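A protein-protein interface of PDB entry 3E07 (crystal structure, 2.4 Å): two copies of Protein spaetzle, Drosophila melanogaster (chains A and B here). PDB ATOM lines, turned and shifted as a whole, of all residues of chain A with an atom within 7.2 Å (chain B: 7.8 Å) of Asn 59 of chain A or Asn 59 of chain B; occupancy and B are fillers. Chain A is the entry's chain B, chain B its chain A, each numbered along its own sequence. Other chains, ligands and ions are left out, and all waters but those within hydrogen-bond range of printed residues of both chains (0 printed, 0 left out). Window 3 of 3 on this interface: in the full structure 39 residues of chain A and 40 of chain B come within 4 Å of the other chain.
O of Asn 59 of chain B sits close to ND2 of Asn 59 of chain A, 2.9 Å away.
O of Leu 9 of chain B lies within hydrogen-bond range of N of Asp 55 of chain B, at 2.8 Å. The backbone carbonyl oxygen (O) of Phe 56 of chain A lies close to the side-chain amide nitrogen (ND2) of Asn 59 of chain A.
Among the printed residues, pairs that only touch across the chains: Phe 56 of chain A with Phe 60 of chain B, Phe 56 of chain A with Pro 61 of chain B, Phe 56 of chain A with Leu 103 of chain B, Phe 60 of chain A with Phe 56 of chain B, Phe 60 of chain A with Asn 59 of chain B, Phe 60 of chain A with Phe 60 of chain B, Tyr 64 of chain A with Phe 56 of chain B, Leu 103 of chain A with Leu 9 of chain B and Leu 103 of chain A with Phe 56 of chain B.
Asn 59 of chain A touches just one residue of chain B: Asn 59 (2.8 Å). Asn 59 of chain B touches just these residues of chain A: Asn 59 (2.8 Å) and Phe 60 (3.2 Å). Printed residues of chain A within 4 Å of Phe 56 of chain B: Phe 60, Tyr 64 and Leu 103. Of the printed residues of chain B, Phe 60 of chain A touches Phe 56 (3.3 Å), Asn 59 (3.2 Å) and Phe 60 (3.6 Å). Of the printed residues of chain B, Phe 56 of chain A touches Phe 60, Pro 61 and Leu 103. Of the printed residues of chain A, Leu 9 of chain B touches Leu 103 (3.8 Å). Pro 61 of chain A touches none of the printed residues of chain B. The nearest printed residue of chain A that does not touch Leu 103 of chain B is Asp 55 of chain A (6.2 Å).
Of the 11 printed residues of chain A, 5 touch a printed residue of chain B. Among the printed residues, 10 pairs touch across the chains. Among the printed residues, no Asp or Glu carboxylate lies within 4 Å of a Lys or Arg side-chain nitrogen of the other chain.
Phe 56 of chain A touches Phe 60 of chain B, and with the chains exchanged Phe 60 of chain A touches Phe 56 of chain B. Phe 56 of chain A touches Pro 61 of chain B, but with the chains exchanged Pro 61 of chain A does not touch Phe 56 of chain B (6.6 Å). Phe 60 of chain A touches Asn 59 of chain B, but with the chains exchanged Asn 59 of chain A does not touch Phe 60 of chain B (4.4 Å). Phe 60 of chain B touches its own counterpart, Phe 60 of chain A. Positions printed for both chains: 55, 56, 57, 58, 59, 60, 61, 62, 66 and 103.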
ATOM      1  N   ASP A  55      22.715  10.529 -22.880  1.00  0.00           N
ATOM      2  CA  ASP A  55      24.047   9.956 -22.906  1.00  0.00           C
ATOM      3  C   ASP A  55      23.995   8.601 -23.602  1.00  0.00           C
ATOM      4  O   ASP A  55      22.997   7.889 -23.503  1.00  0.00           O
ATOM      5  CB  ASP A  55      24.559   9.808 -21.477  1.00  0.00           C
ATOM      6  CG  ASP A  55      24.586  11.135 -20.734  1.00  0.00           C
ATOM      7  OD1 ASP A  55      24.840  11.124 -19.511  1.00  0.00           O
ATOM      8  OD2 ASP A  55      24.357  12.189 -21.373  1.00  0.00           O
ATOM      9  N   PHE A  56      25.064   8.259 -24.317  1.00  0.00           N
ATOM     10  CA  PHE A  56      25.160   6.989 -25.044  1.00  0.00           C
ATOM     11  C   PHE A  56      24.181   6.861 -26.212  1.00  0.00           C
ATOM     12  O   PHE A  56      23.924   5.754 -26.683  1.00  0.00           O
ATOM     13  CB  PHE A  56      24.967   5.795 -24.092  1.00  0.00           C
ATOM     14  CG  PHE A  56      26.007   5.703 -23.009  1.00  0.00           C
ATOM     15  CD1 PHE A  56      25.766   6.232 -21.747  1.00  0.00           C
ATOM     16  CD2 PHE A  56      27.245   5.120 -23.263  1.00  0.00           C
ATOM     17  CE1 PHE A  56      26.740   6.184 -20.754  1.00  0.00           C
ATOM     18  CE2 PHE A  56      28.227   5.070 -22.276  1.00  0.00           C
ATOM     19  CZ  PHE A  56      27.972   5.604 -21.019  1.00  0.00           C
ATOM     20  N   ALA A  57      23.646   7.985 -26.681  1.00  0.00           N
ATOM     21  CA  ALA A  57      22.697   7.980 -27.793  1.00  0.00           C
ATOM     22  C   ALA A  57      23.315   7.361 -29.046  1.00  0.00           C
ATOM     23  O   ALA A  57      22.639   6.662 -29.811  1.00  0.00           O
ATOM     24  CB  ALA A  57      22.237   9.404 -28.089  1.00  0.00           C
ATOM     25  N   ALA A  58      24.606   7.626 -29.241  1.00  0.00           N
ATOM     26  CA  ALA A  58      25.355   7.120 -30.387  1.00  0.00           C
ATOM     27  C   ALA A  58      25.343   5.595 -30.447  1.00  0.00           C
ATOM     28  O   ALA A  58      25.606   5.007 -31.498  1.00  0.00           O
ATOM     29  CB  ALA A  58      26.793   7.629 -30.328  1.00  0.00           C
ATOM     30  N   ASN A  59      25.041   4.961 -29.317  1.00  0.00           N
ATOM     31  CA  ASN A  59      24.991   3.505 -29.246  1.00  0.00           C
ATOM     32  C   ASN A  59      23.651   2.972 -29.733  1.00  0.00           C
ATOM     33  O   ASN A  59      23.445   1.762 -29.803  1.00  0.00           O
ATOM     34  CB  ASN A  59      25.224   3.025 -27.814  1.00  0.00           C
ATOM     35  CG  ASN A  59      26.517   3.541 -27.231  1.00  0.00           C
ATOM     36  OD1 ASN A  59      27.483   3.786 -27.953  1.00  0.00           O
ATOM     37  ND2 ASN A  59      26.551   3.693 -25.910  1.00  0.00           N
ATOM     38  N   PHE A  60      22.741   3.883 -30.057  1.00  0.00           N
ATOM     39  CA  PHE A  60      21.419   3.517 -30.545  1.00  0.00           C
ATOM     40  C   PHE A  60      21.281   3.973 -31.991  1.00  0.00           C
ATOM     41  O   PHE A  60      21.861   4.987 -32.388  1.00  0.00           O
ATOM     42  CB  PHE A  60      20.335   4.201 -29.707  1.00  0.00           C
ATOM     43  CG  PHE A  60      20.237   3.689 -28.300  1.00  0.00           C
ATOM     44  CD1 PHE A  60      19.376   2.653 -27.986  1.00  0.00           C
ATOM     45  CD2 PHE A  60      21.016   4.240 -27.290  1.00  0.00           C
ATOM     46  CE1 PHE A  60      19.294   2.165 -26.691  1.00  0.00           C
ATOM     47  CE2 PHE A  60      20.943   3.757 -25.984  1.00  0.00           C
ATOM     48  CZ  PHE A  60      20.079   2.719 -25.684  1.00  0.00           C
ATOM     49  N   PRO A  61      20.514   3.229 -32.804  1.00  0.00           N
ATOM     50  CA  PRO A  61      20.346   3.635 -34.200  1.00  0.00           C
ATOM     51  C   PRO A  61      19.804   5.057 -34.177  1.00  0.00           C
ATOM     52  O   PRO A  61      19.027   5.410 -33.288  1.00  0.00           O
ATOM     53  CB  PRO A  61      19.323   2.631 -34.726  1.00  0.00           C
ATOM     54  CG  PRO A  61      19.608   1.405 -33.900  1.00  0.00           C
ATOM     55  CD  PRO A  61      19.761   1.994 -32.523  1.00  0.00           C
ATOM     56  N   GLN A  62      20.218   5.888 -35.123  1.00  0.00           N
ATOM     57  CA  GLN A  62      19.719   7.249 -35.129  1.00  0.00           C
ATOM     58  C   GLN A  62      18.243   7.204 -35.452  1.00  0.00           C
ATOM     59  O   GLN A  62      17.553   8.221 -35.403  1.00  0.00           O
ATOM     60  CB  GLN A  62      20.489   8.104 -36.131  1.00  0.00           C
ATOM     61  CG  GLN A  62      21.971   8.176 -35.798  1.00  0.00           C
ATOM     62  CD  GLN A  62      22.686   9.297 -36.517  1.00  0.00           C
ATOM     63  OE1 GLN A  62      22.646   9.389 -37.745  1.00  0.00           O
ATOM     64  NE2 GLN A  62      23.352  10.157 -35.755  1.00  0.00           N
ATOM     65  N   TYR A  64      15.751   5.911 -33.726  1.00  0.00           N
ATOM     66  CA  TYR A  64      15.050   6.460 -32.576  1.00  0.00           C
ATOM     67  C   TYR A  64      15.972   7.406 -31.829  1.00  0.00           C
ATOM     68  O   TYR A  64      16.664   7.000 -30.902  1.00  0.00           O
ATOM     69  CB  TYR A  64      14.549   5.367 -31.613  1.00  0.00           C
ATOM     70  CG  TYR A  64      15.293   4.047 -31.623  1.00  0.00           C
ATOM     71  CD1 TYR A  64      14.927   3.028 -32.507  1.00  0.00           C
ATOM     72  CD2 TYR A  64      16.309   3.785 -30.705  1.00  0.00           C
ATOM     73  CE1 TYR A  64      15.548   1.778 -32.471  1.00  0.00           C
ATOM     74  CE2 TYR A  64      16.938   2.538 -30.661  1.00  0.00           C
ATOM     75  CZ  TYR A  64      16.549   1.538 -31.546  1.00  0.00           C
ATOM     76  OH  TYR A  64      17.156   0.303 -31.502  1.00  0.00           O
ATOM     77  N   PRO A  66      17.306   9.263 -29.258  1.00  0.00           N
ATOM     78  CA  PRO A  66      17.094   9.300 -27.807  1.00  0.00           C
ATOM     79  C   PRO A  66      17.222  10.714 -27.256  1.00  0.00           C
ATOM     80  O   PRO A  66      18.287  11.324 -27.336  1.00  0.00           O
ATOM     81  CB  PRO A  66      18.196   8.379 -27.267  1.00  0.00           C
ATOM     82  CG  PRO A  66      18.606   7.542 -28.471  1.00  0.00           C
ATOM     83  CD  PRO A  66      18.560   8.558 -29.570  1.00  0.00           C
ATOM     84  N   LEU A 103      12.747   7.075 -26.447  1.00  0.00           N
ATOM     85  CA  LEU A 103      13.169   6.533 -27.732  1.00  0.00           C
ATOM     86  C   LEU A 103      12.032   6.554 -28.743  1.00  0.00           C
ATOM     87  O   LEU A 103      10.881   6.292 -28.400  1.00  0.00           O
ATOM     88  CB  LEU A 103      13.655   5.091 -27.565  1.00  0.00           C
ATOM     89  CG  LEU A 103      14.882   4.870 -26.683  1.00  0.00           C
ATOM     90  CD1 LEU A 103      15.212   3.394 -26.667  1.00  0.00           C
ATOM     91  CD2 LEU A 103      16.060   5.667 -27.212  1.00  0.00           C
ATOM     92  N   LEU B   9      13.168   3.029 -21.777  1.00  0.00           N
ATOM     93  CA  LEU B   9      14.012   1.883 -21.438  1.00  0.00           C
ATOM     94  C   LEU B   9      13.462   1.017 -20.307  1.00  0.00           C
ATOM     95  O   LEU B   9      13.854  -0.140 -20.145  1.00  0.00           O
ATOM     96  CB  LEU B   9      15.413   2.377 -21.080  1.00  0.00           C
ATOM     97  CG  LEU B   9      16.112   3.125 -22.219  1.00  0.00           C
ATOM     98  CD1 LEU B   9      17.343   3.812 -21.698  1.00  0.00           C
ATOM     99  CD2 LEU B   9      16.465   2.154 -23.327  1.00  0.00           C
ATOM    100  N   ASP B  55      15.691  -2.001 -21.104  1.00  0.00           N
ATOM    101  CA  ASP B  55      15.677  -2.531 -22.460  1.00  0.00           C
ATOM    102  C   ASP B  55      16.935  -1.968 -23.122  1.00  0.00           C
ATOM    103  O   ASP B  55      17.476  -0.956 -22.669  1.00  0.00           O
ATOM    104  CB  ASP B  55      14.437  -2.066 -23.237  1.00  0.00           C
ATOM    105  CG  ASP B  55      13.140  -2.628 -22.671  1.00  0.00           C
ATOM    106  OD1 ASP B  55      13.169  -3.721 -22.057  1.00  0.00           O
ATOM    107  OD2 ASP B  55      12.086  -1.977 -22.858  1.00  0.00           O
ATOM    108  N   PHE B  56      17.406  -2.616 -24.183  1.00  0.00           N
ATOM    109  CA  PHE B  56      18.592  -2.143 -24.895  1.00  0.00           C
ATOM    110  C   PHE B  56      19.828  -1.989 -24.011  1.00  0.00           C
ATOM    111  O   PHE B  56      20.654  -1.112 -24.253  1.00  0.00           O
ATOM    112  CB  PHE B  56      18.302  -0.802 -25.570  1.00  0.00           C
ATOM    113  CG  PHE B  56      17.112  -0.828 -26.471  1.00  0.00           C
ATOM    114  CD1 PHE B  56      15.941  -0.162 -26.118  1.00  0.00           C
ATOM    115  CD2 PHE B  56      17.144  -1.548 -27.663  1.00  0.00           C
ATOM    116  CE1 PHE B  56      14.811  -0.216 -26.943  1.00  0.00           C
ATOM    117  CE2 PHE B  56      16.025  -1.610 -28.494  1.00  0.00           C
ATOM    118  CZ  PHE B  56      14.855  -0.943 -28.134  1.00  0.00           C
ATOM    119  N   ALA B  57      19.956  -2.844 -23.000  1.00  0.00           N
ATOM    120  CA  ALA B  57      21.100  -2.800 -22.093  1.00  0.00           C
ATOM    121  C   ALA B  57      22.405  -3.126 -22.819  1.00  0.00           C
ATOM    122  O   ALA B  57      23.486  -2.733 -22.385  1.00  0.00           O
ATOM    123  CB  ALA B  57      20.889  -3.777 -20.949  1.00  0.00           C
ATOM    124  N   ALA B  58      22.292  -3.847 -23.929  1.00  0.00           N
ATOM    125  CA  ALA B  58      23.454  -4.234 -24.719  1.00  0.00           C
ATOM    126  C   ALA B  58      24.083  -3.043 -25.438  1.00  0.00           C
ATOM    127  O   ALA B  58      25.229  -3.113 -25.880  1.00  0.00           O
ATOM    128  CB  ALA B  58      23.053  -5.285 -25.723  1.00  0.00           C
ATOM    129  N   ASN B  59      23.332  -1.952 -25.546  1.00  0.00           N
ATOM    130  CA  ASN B  59      23.817  -0.756 -26.221  1.00  0.00           C
ATOM    131  C   ASN B  59      24.688   0.094 -25.313  1.00  0.00           C
ATOM    132  O   ASN B  59      25.183   1.140 -25.710  1.00  0.00           O
ATOM    133  CB  ASN B  59      22.634   0.070 -26.721  1.00  0.00           C
ATOM    134  CG  ASN B  59      21.855  -0.636 -27.803  1.00  0.00           C
ATOM    135  OD1 ASN B  59      21.862  -1.865 -27.889  1.00  0.00           O
ATOM    136  ND2 ASN B  59      21.161   0.134 -28.626  1.00  0.00           N
ATOM    137  N   PHE B  60      24.867  -0.359 -24.082  1.00  0.00           N
ATOM    138  CA  PHE B  60      25.690   0.366 -23.130  1.00  0.00           C
ATOM    139  C   PHE B  60      26.966  -0.419 -22.880  1.00  0.00           C
ATOM    140  O   PHE B  60      26.976  -1.657 -22.985  1.00  0.00           O
ATOM    141  CB  PHE B  60      24.931   0.544 -21.822  1.00  0.00           C
ATOM    142  CG  PHE B  60      23.652   1.299 -21.972  1.00  0.00           C
ATOM    143  CD1 PHE B  60      23.662   2.671 -22.155  1.00  0.00           C
ATOM    144  CD2 PHE B  60      22.436   0.636 -21.951  1.00  0.00           C
ATOM    145  CE1 PHE B  60      22.473   3.374 -22.308  1.00  0.00           C
ATOM    146  CE2 PHE B  60      21.249   1.328 -22.104  1.00  0.00           C
ATOM    147  CZ  PHE B  60      21.264   2.698 -22.282  1.00  0.00           C
ATOM    148  N   PRO B  61      28.060   0.284 -22.540  1.00  0.00           N
ATOM    149  CA  PRO B  61      29.358  -0.353 -22.266  1.00  0.00           C
ATOM    150  C   PRO B  61      29.154  -1.522 -21.298  1.00  0.00           C
ATOM    151  O   PRO B  61      28.494  -1.376 -20.265  1.00  0.00           O
ATOM    152  CB  PRO B  61      30.177   0.784 -21.653  1.00  0.00           C
ATOM    153  CG  PRO B  61      29.605   2.018 -22.327  1.00  0.00           C
ATOM    154  CD  PRO B  61      28.113   1.734 -22.284  1.00  0.00           C
ATOM    155  N   GLN B  62      29.725  -2.676 -21.617  1.00  0.00           N
ATOM    156  CA  GLN B  62      29.533  -3.853 -20.785  1.00  0.00           C
ATOM    157  C   GLN B  62      29.978  -3.779 -19.319  1.00  0.00           C
ATOM    158  O   GLN B  62      29.604  -4.642 -18.523  1.00  0.00           O
ATOM    159  CB  GLN B  62      30.150  -5.079 -21.468  1.00  0.00           C
ATOM    160  CG  GLN B  62      29.575  -6.390 -20.949  1.00  0.00           C
ATOM    161  CD  GLN B  62      29.993  -7.585 -21.774  1.00  0.00           C
ATOM    162  OE1 GLN B  62      31.170  -7.950 -21.809  1.00  0.00           O
ATOM    163  NE2 GLN B  62      29.028  -8.202 -22.452  1.00  0.00           N
ATOM    164  N   PRO B  66      22.891  -1.782 -16.440  1.00  0.00           N
ATOM    165  CA  PRO B  66      21.671  -0.973 -16.563  1.00  0.00           C
ATOM    166  C   PRO B  66      20.449  -1.635 -15.931  1.00  0.00           C
ATOM    167  O   PRO B  66      19.913  -2.608 -16.465  1.00  0.00           O
ATOM    168  CB  PRO B  66      21.499  -0.808 -18.079  1.00  0.00           C
ATOM    169  CG  PRO B  66      22.844  -1.375 -18.695  1.00  0.00           C
ATOM    170  CD  PRO B  66      23.224  -2.431 -17.720  1.00  0.00           C
ATOM    171  N   LEU B 103      22.537   3.231 -14.662  1.00  0.00           N
ATOM    172  CA  LEU B 103      23.696   2.467 -15.075  1.00  0.00           C
ATOM    173  C   LEU B 103      24.606   2.276 -13.865  1.00  0.00           C
ATOM    174  O   LEU B 103      25.340   3.185 -13.491  1.00  0.00           O
ATOM    175  CB  LEU B 103      24.440   3.209 -16.194  1.00  0.00           C
ATOM    176  CG  LEU B 103      23.606   3.650 -17.408  1.00  0.00           C
ATOM    177  CD1 LEU B 103      24.496   4.428 -18.332  1.00  0.00           C
ATOM    178  CD2 LEU B 103      23.006   2.466 -18.134  1.00  0.00           C
